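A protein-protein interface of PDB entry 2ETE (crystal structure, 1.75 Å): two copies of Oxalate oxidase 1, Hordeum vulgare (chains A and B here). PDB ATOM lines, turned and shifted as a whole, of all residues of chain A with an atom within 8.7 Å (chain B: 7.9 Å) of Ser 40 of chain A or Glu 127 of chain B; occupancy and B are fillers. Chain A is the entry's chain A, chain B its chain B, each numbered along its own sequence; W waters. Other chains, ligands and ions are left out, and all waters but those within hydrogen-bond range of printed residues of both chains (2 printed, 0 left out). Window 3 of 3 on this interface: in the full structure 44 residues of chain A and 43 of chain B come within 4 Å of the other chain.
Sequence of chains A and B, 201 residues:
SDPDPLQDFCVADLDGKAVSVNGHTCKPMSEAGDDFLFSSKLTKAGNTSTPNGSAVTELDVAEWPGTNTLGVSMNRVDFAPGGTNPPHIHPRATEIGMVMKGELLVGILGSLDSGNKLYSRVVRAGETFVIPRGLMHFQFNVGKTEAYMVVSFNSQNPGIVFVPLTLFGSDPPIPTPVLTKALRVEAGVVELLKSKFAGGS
Hydrophobic or aromatic side chains of chain A that line the printed part of chain B: Phe 38, Leu 42, Leu 59, Trp 64, Met 74 and Val 150. Among the printed residues, no Asp or Glu carboxylate lies within 4 Å of a Lys or Arg side-chain nitrogen of the other chain.
N of Thr 128 of chain B is in hydrogen-bond range of O of Ser 39 of chain A (2.9 Å).
Phe 129 of chain B touches Leu 37 of chain A (CA to O, 3.2 Å). CA of Phe 38 of chain A touches O of Thr 128 of chain B, at 3.4 Å. Phe 38 of chain A touches Phe 129 of chain B. CG2 of Thr 43 of chain A touches C of Gly 126 of chain B, at 3.6 Å. Thr 43 of chain A touches Glu 127 of chain B. Thr 128 of chain B touches Leu 59 of chain A (OG1 to CD2, 3.7 Å). CH2 of Trp 64 of chain A touches OG1 of Thr 128 of chain B (3.4 Å). Phe 129 of chain B touches Trp 64 of chain A (C to CH2, 3.5 Å). Thr 128 of chain B touches Met 74 of chain A (CG2 to SD, 3.7 Å). Val 150 of chain A touches Met 98 of chain B (CG1 to CE, 3.8 Å).
Water W1 lies within hydrogen-bond range of the backbone carbonyl oxygen (O) of Gly 126 of chain B (2.7 Å), the backbone NH (N) of Leu 42 of chain A (3.0 Å), the backbone carbonyl oxygen (O) of Ser 39 of chain A (3.2 Å) and the backbone NH (N) of Lys 41 of chain A (3.3 Å). Water W2 lies within hydrogen-bond range of NH1 of Arg 121 of chain B (2.8 Å), O of Thr 128 of chain B (3.0 Å) and O of Ser 39 of chain A (3.2 Å).
The backbone carbonyl oxygen (O) of Ser 40 of chain A sits at hydrogen-bond distance from the side-chain hydroxyl (OG1) of Thr 43 of chain A. NH1 of Arg 76 of chain A lies within hydrogen-bond range of O of Leu 42 of chain A (3.0 Å). N of Leu 59 of chain A lies within hydrogen-bond range of O of Met 74 of chain A (2.9 Å). N of Gly 97 of chain B lies within hydrogen-bond range of O of Phe 129 of chain B (3.0 Å). O of Val 99 of chain B sits at hydrogen-bond distance from N of Gly 126 of chain B, at 2.9 Å. The backbone carbonyl oxygen of Glu 127 of chain B lies within hydrogen-bond range of the backbone NH of Val 99 of chain B, at 3.1 Å.
1 position is printed for both chains. Of the 18 pairs that touch across the chains among the printed residues, none has its exchanged pair printed and touching as well.
Ser 39 of chain A touches just these residues of chain B: Glu 127 and Thr 128. Ser 40 of chain A touches just one residue of chain B: Glu 127 (3.5 Å). Printed residues of chain B within 4 Å of Leu 42 of chain A: Met 98 (3.8 Å) and Gly 126 (3.7 Å). Printed residues of chain B within 4 Å of Thr 43 of chain A: Ala 125, Gly 126 and Glu 127. Of the printed residues of chain A, Met 98 of chain B touches Leu 42 and Val 150. Val 122 of chain B touches none of the printed residues of chain A. Of chain A, only Leu 42 and Thr 43 come within 4 Å of Gly 126 of chain B. Of chain A, only Ser 39 (3.5 Å), Ser 40 (3.5 Å) and Thr 43 (3.6 Å) come within 4 Å of Glu 127 of chain B. Printed residues of chain A within 4 Å of Thr 128 of chain B: Phe 38, Ser 39, Leu 59, Trp 64 and Met 74. Met 149 of chain B touches none of the printed residues of chain A. The nearest printed residue of chain B that does not touch Leu 37 of chain A is Thr 128 of chain B (4.2 Å).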
ATOM      1  N   ASP A  35     -12.724 -29.509  -5.908  1.00  0.00           N
ATOM      2  CA  ASP A  35     -12.435 -28.135  -5.478  1.00  0.00           C
ATOM      3  C   ASP A  35     -11.311 -28.002  -4.448  1.00  0.00           C
ATOM      4  O   ASP A  35     -11.060 -26.896  -3.950  1.00  0.00           O
ATOM      5  CB  ASP A  35     -13.704 -27.482  -4.911  1.00  0.00           C
ATOM      6  CG  ASP A  35     -14.853 -27.461  -5.905  1.00  0.00           C
ATOM      7  OD1 ASP A  35     -14.593 -27.429  -7.128  1.00  0.00           O
ATOM      8  OD2 ASP A  35     -16.020 -27.474  -5.458  1.00  0.00           O
ATOM      9  N   LEU A  37      -8.100 -27.943  -4.473  1.00  0.00           N
ATOM     10  CA  LEU A  37      -6.956 -27.077  -4.782  1.00  0.00           C
ATOM     11  C   LEU A  37      -7.270 -25.582  -4.645  1.00  0.00           C
ATOM     12  O   LEU A  37      -6.426 -24.738  -4.958  1.00  0.00           O
ATOM     13  CB  LEU A  37      -6.419 -27.377  -6.193  1.00  0.00           C
ATOM     14  CG  LEU A  37      -5.848 -28.785  -6.409  1.00  0.00           C
ATOM     15  CD1 LEU A  37      -5.556 -29.041  -7.884  1.00  0.00           C
ATOM     16  CD2 LEU A  37      -4.592 -29.030  -5.552  1.00  0.00           C
ATOM     17  N   PHE A  38      -8.475 -25.259  -4.172  1.00  0.00           N
ATOM     18  CA  PHE A  38      -8.963 -23.875  -4.140  1.00  0.00           C
ATOM     19  C   PHE A  38      -9.568 -23.507  -2.784  1.00  0.00           C
ATOM     20  O   PHE A  38     -10.149 -24.360  -2.106  1.00  0.00           O
ATOM     21  CB  PHE A  38     -10.019 -23.657  -5.233  1.00  0.00           C
ATOM     22  CG  PHE A  38      -9.550 -24.011  -6.615  1.00  0.00           C
ATOM     23  CD1 PHE A  38      -9.910 -25.228  -7.197  1.00  0.00           C
ATOM     24  CD2 PHE A  38      -8.752 -23.128  -7.341  1.00  0.00           C
ATOM     25  CE1 PHE A  38      -9.471 -25.569  -8.482  1.00  0.00           C
ATOM     26  CE2 PHE A  38      -8.308 -23.459  -8.627  1.00  0.00           C
ATOM     27  CZ  PHE A  38      -8.669 -24.682  -9.196  1.00  0.00           C
ATOM     28  N   SER A  39      -9.439 -22.237  -2.402  1.00  0.00           N
ATOM     29  CA  SER A  39     -10.088 -21.717  -1.187  1.00  0.00           C
ATOM     30  C   SER A  39     -10.581 -20.279  -1.351  1.00  0.00           C
ATOM     31  O   SER A  39     -10.032 -19.510  -2.144  1.00  0.00           O
ATOM     32  CB  SER A  39      -9.144 -21.817   0.021  1.00  0.00           C
ATOM     33  OG  SER A  39      -9.804 -21.443   1.227  1.00  0.00           O
ATOM     34  N   SER A  40     -11.620 -19.925  -0.596  1.00  0.00           N
ATOM     35  CA  SER A  40     -12.130 -18.553  -0.564  1.00  0.00           C
ATOM     36  C   SER A  40     -12.089 -17.972   0.856  1.00  0.00           C
ATOM     37  O   SER A  40     -12.644 -16.903   1.114  1.00  0.00           O
ATOM     38  CB  SER A  40     -13.555 -18.500  -1.128  1.00  0.00           C
ATOM     39  OG  SER A  40     -14.460 -19.184  -0.278  1.00  0.00           O
ATOM     40  N   LYS A  41     -11.415 -18.668   1.769  1.00  0.00           N
ATOM     41  CA  LYS A  41     -11.443 -18.290   3.191  1.00  0.00           C
ATOM     42  C   LYS A  41     -10.770 -16.953   3.528  1.00  0.00           C
ATOM     43  O   LYS A  41     -11.052 -16.366   4.575  1.00  0.00           O
ATOM     44  CB  LYS A  41     -10.904 -19.422   4.078  1.00  0.00           C
ATOM     45  CG  LYS A  41     -11.861 -20.613   4.183  1.00  0.00           C
ATOM     46  CD  LYS A  41     -11.380 -21.660   5.179  1.00  0.00           C
ATOM     47  CE  LYS A  41     -12.392 -22.793   5.302  1.00  0.00           C
ATOM     48  NZ  LYS A  41     -11.859 -23.930   6.120  1.00  0.00           N
ATOM     49  N   LEU A  42      -9.902 -16.457   2.646  1.00  0.00           N
ATOM     50  CA  LEU A  42      -9.189 -15.203   2.921  1.00  0.00           C
ATOM     51  C   LEU A  42      -9.806 -13.963   2.263  1.00  0.00           C
ATOM     52  O   LEU A  42      -9.196 -12.893   2.269  1.00  0.00           O
ATOM     53  CB  LEU A  42      -7.701 -15.322   2.554  1.00  0.00           C
ATOM     54  CG  LEU A  42      -6.911 -16.483   3.173  1.00  0.00           C
ATOM     55  CD1 LEU A  42      -5.447 -16.398   2.772  1.00  0.00           C
ATOM     56  CD2 LEU A  42      -7.051 -16.522   4.701  1.00  0.00           C
ATOM     57  N   THR A  43     -11.013 -14.104   1.717  1.00  0.00           N
ATOM     58  CA  THR A  43     -11.684 -12.987   1.044  1.00  0.00           C
ATOM     59  C   THR A  43     -12.159 -11.897   2.002  1.00  0.00           C
ATOM     60  O   THR A  43     -12.365 -10.757   1.589  1.00  0.00           O
ATOM     61  CB  THR A  43     -12.904 -13.442   0.214  1.00  0.00           C
ATOM     62  OG1 THR A  43     -13.819 -14.164   1.050  1.00  0.00           O
ATOM     63  CG2 THR A  43     -12.468 -14.303  -0.961  1.00  0.00           C
ATOM     64  N   LYS A  44     -12.342 -12.249   3.270  1.00  0.00           N
ATOM     65  CA  LYS A  44     -12.894 -11.304   4.237  1.00  0.00           C
ATOM     66  C   LYS A  44     -11.927 -10.958   5.365  1.00  0.00           C
ATOM     67  O   LYS A  44     -11.169 -11.811   5.832  1.00  0.00           O
ATOM     68  CB  LYS A  44     -14.226 -11.824   4.780  1.00  0.00           C
ATOM     69  CG  LYS A  44     -15.351 -11.730   3.754  1.00  0.00           C
ATOM     70  CD  LYS A  44     -16.490 -12.688   4.056  1.00  0.00           C
ATOM     71  CE  LYS A  44     -17.402 -12.828   2.844  1.00  0.00           C
ATOM     72  NZ  LYS A  44     -18.592 -13.682   3.120  1.00  0.00           N
ATOM     73  N   ALA A  45     -11.964  -9.695   5.784  1.00  0.00           N
ATOM     74  CA  ALA A  45     -11.114  -9.195   6.866  1.00  0.00           C
ATOM     75  C   ALA A  45     -11.494  -9.794   8.219  1.00  0.00           C
ATOM     76  O   ALA A  45     -12.679  -9.978   8.521  1.00  0.00           O
ATOM     77  CB  ALA A  45     -11.173  -7.670   6.923  1.00  0.00           C
ATOM     78  N   THR A  57      -6.257 -14.814  10.127  1.00  0.00           N
ATOM     79  CA  THR A  57      -7.154 -15.774   9.485  1.00  0.00           C
ATOM     80  C   THR A  57      -6.271 -16.830   8.825  1.00  0.00           C
ATOM     81  O   THR A  57      -5.599 -16.555   7.832  1.00  0.00           O
ATOM     82  CB  THR A  57      -8.094 -15.096   8.453  1.00  0.00           C
ATOM     83  OG1 THR A  57      -8.835 -14.050   9.097  1.00  0.00           O
ATOM     84  CG2 THR A  57      -9.077 -16.102   7.865  1.00  0.00           C
ATOM     85  N   LEU A  59      -4.807 -20.180   6.928  1.00  0.00           N
ATOM     86  CA  LEU A  59      -5.070 -21.098   5.833  1.00  0.00           C
ATOM     87  C   LEU A  59      -3.965 -22.151   5.794  1.00  0.00           C
ATOM     88  O   LEU A  59      -3.330 -22.393   4.762  1.00  0.00           O
ATOM     89  CB  LEU A  59      -5.229 -20.351   4.504  1.00  0.00           C
ATOM     90  CG  LEU A  59      -6.199 -20.971   3.496  1.00  0.00           C
ATOM     91  CD1 LEU A  59      -7.579 -21.236   4.114  1.00  0.00           C
ATOM     92  CD2 LEU A  59      -6.332 -20.088   2.258  1.00  0.00           C
ATOM     93  N   GLU A  63      -7.247 -25.794   7.746  1.00  0.00           N
ATOM     94  CA  GLU A  63      -8.268 -24.965   7.097  1.00  0.00           C
ATOM     95  C   GLU A  63      -8.325 -25.169   5.580  1.00  0.00           C
ATOM     96  O   GLU A  63      -9.336 -24.847   4.942  1.00  0.00           O
ATOM     97  CB  GLU A  63      -8.036 -23.484   7.421  1.00  0.00           C
ATOM     98  CG  GLU A  63      -8.276 -23.121   8.889  1.00  0.00           C
ATOM     99  CD  GLU A  63      -9.734 -23.256   9.309  1.00  0.00           C
ATOM    100  OE1 GLU A  63     -10.630 -22.875   8.529  1.00  0.00           O
ATOM    101  OE2 GLU A  63      -9.980 -23.736  10.434  1.00  0.00           O
ATOM    102  N   TRP A  64      -7.237 -25.700   5.019  1.00  0.00           N
ATOM    103  CA  TRP A  64      -7.124 -25.960   3.581  1.00  0.00           C
ATOM    104  C   TRP A  64      -6.483 -27.340   3.390  1.00  0.00           C
ATOM    105  O   TRP A  64      -5.290 -27.437   3.081  1.00  0.00           O
ATOM    106  CB  TRP A  64      -6.272 -24.873   2.907  1.00  0.00           C
ATOM    107  CG  TRP A  64      -6.366 -24.819   1.392  1.00  0.00           C
ATOM    108  CD1 TRP A  64      -7.078 -25.656   0.573  1.00  0.00           C
ATOM    109  CD2 TRP A  64      -5.695 -23.890   0.525  1.00  0.00           C
ATOM    110  NE1 TRP A  64      -6.908 -25.289  -0.746  1.00  0.00           N
ATOM    111  CE2 TRP A  64      -6.061 -24.215  -0.803  1.00  0.00           C
ATOM    112  CE3 TRP A  64      -4.820 -22.818   0.742  1.00  0.00           C
ATOM    113  CZ2 TRP A  64      -5.586 -23.496  -1.910  1.00  0.00           C
ATOM    114  CZ3 TRP A  64      -4.356 -22.097  -0.359  1.00  0.00           C
ATOM    115  CH2 TRP A  64      -4.735 -22.446  -1.668  1.00  0.00           C
ATOM    116  N   MET A  74      -0.863 -20.601   3.678  1.00  0.00           N
ATOM    117  CA  MET A  74      -0.989 -19.144   3.686  1.00  0.00           C
ATOM    118  C   MET A  74      -1.714 -18.674   4.932  1.00  0.00           C
ATOM    119  O   MET A  74      -2.362 -19.465   5.617  1.00  0.00           O
ATOM    120  CB  MET A  74      -1.792 -18.670   2.472  1.00  0.00           C
ATOM    121  CG  MET A  74      -1.112 -18.808   1.144  1.00  0.00           C
ATOM    122  SD  MET A  74      -2.258 -18.367  -0.185  1.00  0.00           S
ATOM    123  CE  MET A  74      -2.278 -16.594  -0.050  1.00  0.00           C
ATOM    124  N   ARG A  76      -3.819 -14.655   6.258  1.00  0.00           N
ATOM    125  CA  ARG A  76      -4.087 -13.233   6.163  1.00  0.00           C
ATOM    126  C   ARG A  76      -4.041 -12.659   7.573  1.00  0.00           C
ATOM    127  O   ARG A  76      -4.478 -13.308   8.523  1.00  0.00           O
ATOM    128  CB  ARG A  76      -5.470 -13.017   5.543  1.00  0.00           C
ATOM    129  CG  ARG A  76      -5.941 -11.583   5.558  1.00  0.00           C
ATOM    130  CD  ARG A  76      -7.324 -11.439   4.946  1.00  0.00           C
ATOM    131  NE  ARG A  76      -7.780 -10.059   5.070  1.00  0.00           N
ATOM    132  CZ  ARG A  76      -8.494  -9.407   4.157  1.00  0.00           C
ATOM    133  NH1 ARG A  76      -8.862 -10.005   3.026  1.00  0.00           N
ATOM    134  NH2 ARG A  76      -8.841  -8.146   4.380  1.00  0.00           N
ATOM    135  N   VAL A 150      -0.971 -10.426   3.337  1.00  0.00           N
ATOM    136  CA  VAL A 150      -1.169 -11.823   2.991  1.00  0.00           C
ATOM    137  C   VAL A 150       0.212 -12.464   2.906  1.00  0.00           C
ATOM    138  O   VAL A 150       1.090 -11.968   2.192  1.00  0.00           O
ATOM    139  CB  VAL A 150      -1.925 -11.969   1.655  1.00  0.00           C
ATOM    140  CG1 VAL A 150      -2.002 -13.430   1.230  1.00  0.00           C
ATOM    141  CG2 VAL A 150      -3.331 -11.377   1.771  1.00  0.00           C
ATOM    142  N   GLY B  97      -1.020 -19.282  -4.567  1.00  0.00           N
ATOM    143  CA  GLY B  97      -1.329 -17.945  -5.063  1.00  0.00           C
ATOM    144  C   GLY B  97      -2.672 -17.363  -4.681  1.00  0.00           C
ATOM    145  O   GLY B  97      -3.584 -18.084  -4.273  1.00  0.00           O
ATOM    146  N   MET B  98      -2.781 -16.045  -4.828  1.00  0.00           N
ATOM    147  CA  MET B  98      -4.029 -15.327  -4.588  1.00  0.00           C
ATOM    148  C   MET B  98      -4.311 -14.372  -5.748  1.00  0.00           C
ATOM    149  O   MET B  98      -3.429 -13.616  -6.167  1.00  0.00           O
ATOM    150  CB  MET B  98      -3.957 -14.543  -3.270  1.00  0.00           C
ATOM    151  CG  MET B  98      -5.195 -13.698  -2.971  1.00  0.00           C
ATOM    152  SD  MET B  98      -5.085 -12.750  -1.433  1.00  0.00           S
ATOM    153  CE  MET B  98      -5.458 -14.017  -0.227  1.00  0.00           C
ATOM    154  N   VAL B  99      -5.539 -14.411  -6.261  1.00  0.00           N
ATOM    155  CA  VAL B  99      -5.990 -13.417  -7.239  1.00  0.00           C
ATOM    156  C   VAL B  99      -6.278 -12.114  -6.491  1.00  0.00           C
ATOM    157  O   VAL B  99      -6.987 -12.118  -5.479  1.00  0.00           O
ATOM    158  CB  VAL B  99      -7.229 -13.914  -8.029  1.00  0.00           C
ATOM    159  CG1 VAL B  99      -7.864 -12.786  -8.857  1.00  0.00           C
ATOM    160  CG2 VAL B  99      -6.832 -15.083  -8.938  1.00  0.00           C
ATOM    161  N   MET B 100      -5.711 -11.012  -6.980  1.00  0.00           N
ATOM    162  CA  MET B 100      -5.856  -9.714  -6.313  1.00  0.00           C
ATOM    163  C   MET B 100      -6.932  -8.823  -6.937  1.00  0.00           C
ATOM    164  O   MET B 100      -7.611  -8.073  -6.227  1.00  0.00           O
ATOM    165  CB  MET B 100      -4.517  -8.968  -6.259  1.00  0.00           C
ATOM    166  CG  MET B 100      -3.429  -9.623  -5.394  1.00  0.00           C
ATOM    167  SD  MET B 100      -3.994 -10.178  -3.767  1.00  0.00           S
ATOM    168  CE  MET B 100      -4.782  -8.710  -3.112  1.00  0.00           C
ATOM    169  N   GLY B 102      -9.798  -8.874 -10.534  1.00  0.00           N
ATOM    170  CA  GLY B 102     -10.339  -9.496 -11.742  1.00  0.00           C
ATOM    171  C   GLY B 102     -10.817 -10.928 -11.585  1.00  0.00           C
ATOM    172  O   GLY B 102     -11.034 -11.405 -10.470  1.00  0.00           O
ATOM    173  N   GLU B 103     -10.982 -11.608 -12.720  1.00  0.00           N
ATOM    174  CA  GLU B 103     -11.522 -12.967 -12.762  1.00  0.00           C
ATOM    175  C   GLU B 103     -10.610 -13.856 -13.603  1.00  0.00           C
ATOM    176  O   GLU B 103     -10.521 -13.684 -14.823  1.00  0.00           O
ATOM    177  CB  GLU B 103     -12.925 -12.970 -13.374  1.00  0.00           C
ATOM    178  CG  GLU B 103     -13.965 -12.140 -12.635  1.00  0.00           C
ATOM    179  CD  GLU B 103     -15.237 -11.976 -13.443  1.00  0.00           C
ATOM    180  OE1 GLU B 103     -16.196 -12.736 -13.201  1.00  0.00           O
ATOM    181  OE2 GLU B 103     -15.270 -11.102 -14.339  1.00  0.00           O
ATOM    182  N   LEU B 104      -9.945 -14.804 -12.947  1.00  0.00           N
ATOM    183  CA  LEU B 104      -8.984 -15.684 -13.612  1.00  0.00           C
ATOM    184  C   LEU B 104      -9.410 -17.140 -13.552  1.00  0.00           C
ATOM    185  O   LEU B 104      -9.534 -17.711 -12.463  1.00  0.00           O
ATOM    186  CB  LEU B 104      -7.587 -15.541 -12.979  1.00  0.00           C
ATOM    187  CG  LEU B 104      -6.774 -14.274 -13.245  1.00  0.00           C
ATOM    188  CD1 LEU B 104      -5.512 -14.277 -12.388  1.00  0.00           C
ATOM    189  CD2 LEU B 104      -6.416 -14.161 -14.718  1.00  0.00           C
ATOM    190  N   VAL B 106      -8.329 -20.638 -13.481  1.00  0.00           N
ATOM    191  CA  VAL B 106      -7.094 -21.296 -13.076  1.00  0.00           C
ATOM    192  C   VAL B 106      -7.278 -22.798 -13.238  1.00  0.00           C
ATOM    193  O   VAL B 106      -8.208 -23.377 -12.675  1.00  0.00           O
ATOM    194  CB  VAL B 106      -6.723 -20.966 -11.602  1.00  0.00           C
ATOM    195  CG1 VAL B 106      -5.432 -21.677 -11.197  1.00  0.00           C
ATOM    196  CG2 VAL B 106      -6.578 -19.453 -11.408  1.00  0.00           C
ATOM    197  N   ARG B 121     -11.379 -23.622 -11.888  1.00  0.00           N
ATOM    198  CA  ARG B 121     -12.479 -22.725 -11.539  1.00  0.00           C
ATOM    199  C   ARG B 121     -12.072 -21.285 -11.820  1.00  0.00           C
ATOM    200  O   ARG B 121     -10.885 -20.992 -11.985  1.00  0.00           O
ATOM    201  CB  ARG B 121     -12.911 -22.901 -10.071  1.00  0.00           C
ATOM    202  CG  ARG B 121     -11.980 -22.309  -9.031  1.00  0.00           C
ATOM    203  CD  ARG B 121     -12.527 -22.512  -7.601  1.00  0.00           C
ATOM    204  NE  ARG B 121     -13.796 -21.822  -7.365  1.00  0.00           N
ATOM    205  CZ  ARG B 121     -13.915 -20.557  -6.952  1.00  0.00           C
ATOM    206  NH1 ARG B 121     -12.840 -19.812  -6.711  1.00  0.00           N
ATOM    207  NH2 ARG B 121     -15.125 -20.031  -6.781  1.00  0.00           N
ATOM    208  N   VAL B 122     -13.060 -20.398 -11.886  1.00  0.00           N
ATOM    209  CA  VAL B 122     -12.800 -18.967 -11.999  1.00  0.00           C
ATOM    210  C   VAL B 122     -12.542 -18.426 -10.593  1.00  0.00           C
ATOM    211  O   VAL B 122     -13.421 -18.485  -9.718  1.00  0.00           O
ATOM    212  CB  VAL B 122     -13.967 -18.217 -12.690  1.00  0.00           C
ATOM    213  CG1 VAL B 122     -13.713 -16.710 -12.700  1.00  0.00           C
ATOM    214  CG2 VAL B 122     -14.172 -18.747 -14.114  1.00  0.00           C
ATOM    215  N   VAL B 123     -11.324 -17.927 -10.392  1.00  0.00           N
ATOM    216  CA  VAL B 123     -10.845 -17.457  -9.092  1.00  0.00           C
ATOM    217  C   VAL B 123     -10.888 -15.927  -9.075  1.00  0.00           C
ATOM    218  O   VAL B 123     -10.369 -15.274  -9.986  1.00  0.00           O
ATOM    219  CB  VAL B 123      -9.407 -17.983  -8.816  1.00  0.00           C
ATOM    220  CG1 VAL B 123      -8.912 -17.558  -7.431  1.00  0.00           C
ATOM    221  CG2 VAL B 123      -9.360 -19.509  -8.949  1.00  0.00           C
ATOM    222  N   ARG B 124     -11.523 -15.368  -8.042  1.00  0.00           N
ATOM    223  CA  ARG B 124     -11.731 -13.917  -7.932  1.00  0.00           C
ATOM    224  C   ARG B 124     -10.934 -13.303  -6.773  1.00  0.00           C
ATOM    225  O   ARG B 124     -10.196 -14.011  -6.081  1.00  0.00           O
ATOM    226  CB  ARG B 124     -13.231 -13.612  -7.814  1.00  0.00           C
ATOM    227  CG  ARG B 124     -13.988 -13.929  -9.099  1.00  0.00           C
ATOM    228  CD  ARG B 124     -15.491 -13.767  -8.961  1.00  0.00           C
ATOM    229  NE  ARG B 124     -16.154 -13.966 -10.252  1.00  0.00           N
ATOM    230  CZ  ARG B 124     -16.496 -15.152 -10.754  1.00  0.00           C
ATOM    231  NH1 ARG B 124     -16.247 -16.270 -10.079  1.00  0.00           N
ATOM    232  NH2 ARG B 124     -17.092 -15.221 -11.937  1.00  0.00           N
ATOM    233  N   ALA B 125     -11.082 -11.992  -6.571  1.00  0.00           N
ATOM    234  CA  ALA B 125     -10.298 -11.252  -5.577  1.00  0.00           C
ATOM    235  C   ALA B 125     -10.341 -11.896  -4.192  1.00  0.00           C
ATOM    236  O   ALA B 125     -11.422 -12.172  -3.658  1.00  0.00           O
ATOM    237  CB  ALA B 125     -10.767  -9.801  -5.499  1.00  0.00           C
ATOM    238  N   GLY B 126      -9.158 -12.143  -3.629  1.00  0.00           N
ATOM    239  CA  GLY B 126      -9.028 -12.733  -2.291  1.00  0.00           C
ATOM    240  C   GLY B 126      -9.069 -14.255  -2.253  1.00  0.00           C
ATOM    241  O   GLY B 126      -8.781 -14.864  -1.213  1.00  0.00           O
ATOM    242  N   GLU B 127      -9.435 -14.873  -3.375  1.00  0.00           N
ATOM    243  CA  GLU B 127      -9.498 -16.334  -3.463  1.00  0.00           C
ATOM    244  C   GLU B 127      -8.140 -16.913  -3.864  1.00  0.00           C
ATOM    245  O   GLU B 127      -7.330 -16.237  -4.504  1.00  0.00           O
ATOM    246  CB  GLU B 127     -10.615 -16.787  -4.413  1.00  0.00           C
ATOM    247  CG  GLU B 127     -11.999 -16.296  -3.980  1.00  0.00           C
ATOM    248  CD  GLU B 127     -13.133 -16.793  -4.858  1.00  0.00           C
ATOM    249  OE1 GLU B 127     -12.994 -16.795  -6.101  1.00  0.00           O
ATOM    250  OE2 GLU B 127     -14.182 -17.175  -4.295  1.00  0.00           O
ATOM    251  N   THR B 128      -7.895 -18.162  -3.479  1.00  0.00           N
ATOM    252  CA  THR B 128      -6.559 -18.753  -3.592  1.00  0.00           C
ATOM    253  C   THR B 128      -6.556 -20.096  -4.323  1.00  0.00           C
ATOM    254  O   THR B 128      -7.602 -20.733  -4.492  1.00  0.00           O
ATOM    255  CB  THR B 128      -5.905 -18.933  -2.197  1.00  0.00           C
ATOM    256  OG1 THR B 128      -6.754 -19.745  -1.374  1.00  0.00           O
ATOM    257  CG2 THR B 128      -5.672 -17.575  -1.519  1.00  0.00           C
ATOM    258  N   PHE B 129      -5.368 -20.514  -4.756  1.00  0.00           N
ATOM    259  CA  PHE B 129      -5.180 -21.798  -5.431  1.00  0.00           C
ATOM    260  C   PHE B 129      -3.798 -22.348  -5.081  1.00  0.00           C
ATOM    261  O   PHE B 129      -2.899 -21.590  -4.697  1.00  0.00           O
ATOM    262  CB  PHE B 129      -5.325 -21.650  -6.958  1.00  0.00           C
ATOM    263  CG  PHE B 129      -4.391 -20.631  -7.566  1.00  0.00           C
ATOM    264  CD1 PHE B 129      -3.096 -20.989  -7.946  1.00  0.00           C
ATOM    265  CD2 PHE B 129      -4.811 -19.315  -7.767  1.00  0.00           C
ATOM    266  CE1 PHE B 129      -2.226 -20.049  -8.501  1.00  0.00           C
ATOM    267  CE2 PHE B 129      -3.951 -18.368  -8.327  1.00  0.00           C
ATOM    268  CZ  PHE B 129      -2.656 -18.736  -8.691  1.00  0.00           C
ATOM    269  N   MET B 149      -2.531 -11.377 -10.158  1.00  0.00           N
ATOM    270  CA  MET B 149      -2.364 -12.292  -9.034  1.00  0.00           C
ATOM    271  C   MET B 149      -0.956 -12.162  -8.460  1.00  0.00           C
ATOM    272  O   MET B 149      -0.030 -11.699  -9.131  1.00  0.00           O
ATOM    273  CB  MET B 149      -2.622 -13.741  -9.472  1.00  0.00           C
ATOM    274  CG  MET B 149      -1.584 -14.307 -10.438  1.00  0.00           C
ATOM    275  SD  MET B 149      -1.996 -15.948 -11.061  1.00  0.00           S
ATOM    276  CE  MET B 149      -0.428 -16.435 -11.752  1.00  0.00           C
ATOM    277  N   VAL B 150      -0.806 -12.570  -7.206  1.00  0.00           N
ATOM    278  CA  VAL B 150       0.501 -12.622  -6.570  1.00  0.00           C
ATOM    279  C   VAL B 150       0.676 -14.040  -6.038  1.00  0.00           C
ATOM    280  O   VAL B 150      -0.201 -14.555  -5.339  1.00  0.00           O
ATOM    281  CB  VAL B 150       0.627 -11.573  -5.440  1.00  0.00           C
ATOM    282  CG1 VAL B 150       1.950 -11.716  -4.718  1.00  0.00           C
ATOM    283  CG2 VAL B 150       0.495 -10.157  -6.007  1.00  0.00           C
HETATM  284  O   HOH W   1      -9.021 -17.344  -0.053  1.00  0.00           O
HETATM  285  O   HOH W   2     -10.489 -20.283  -5.243  1.00  0.00           O
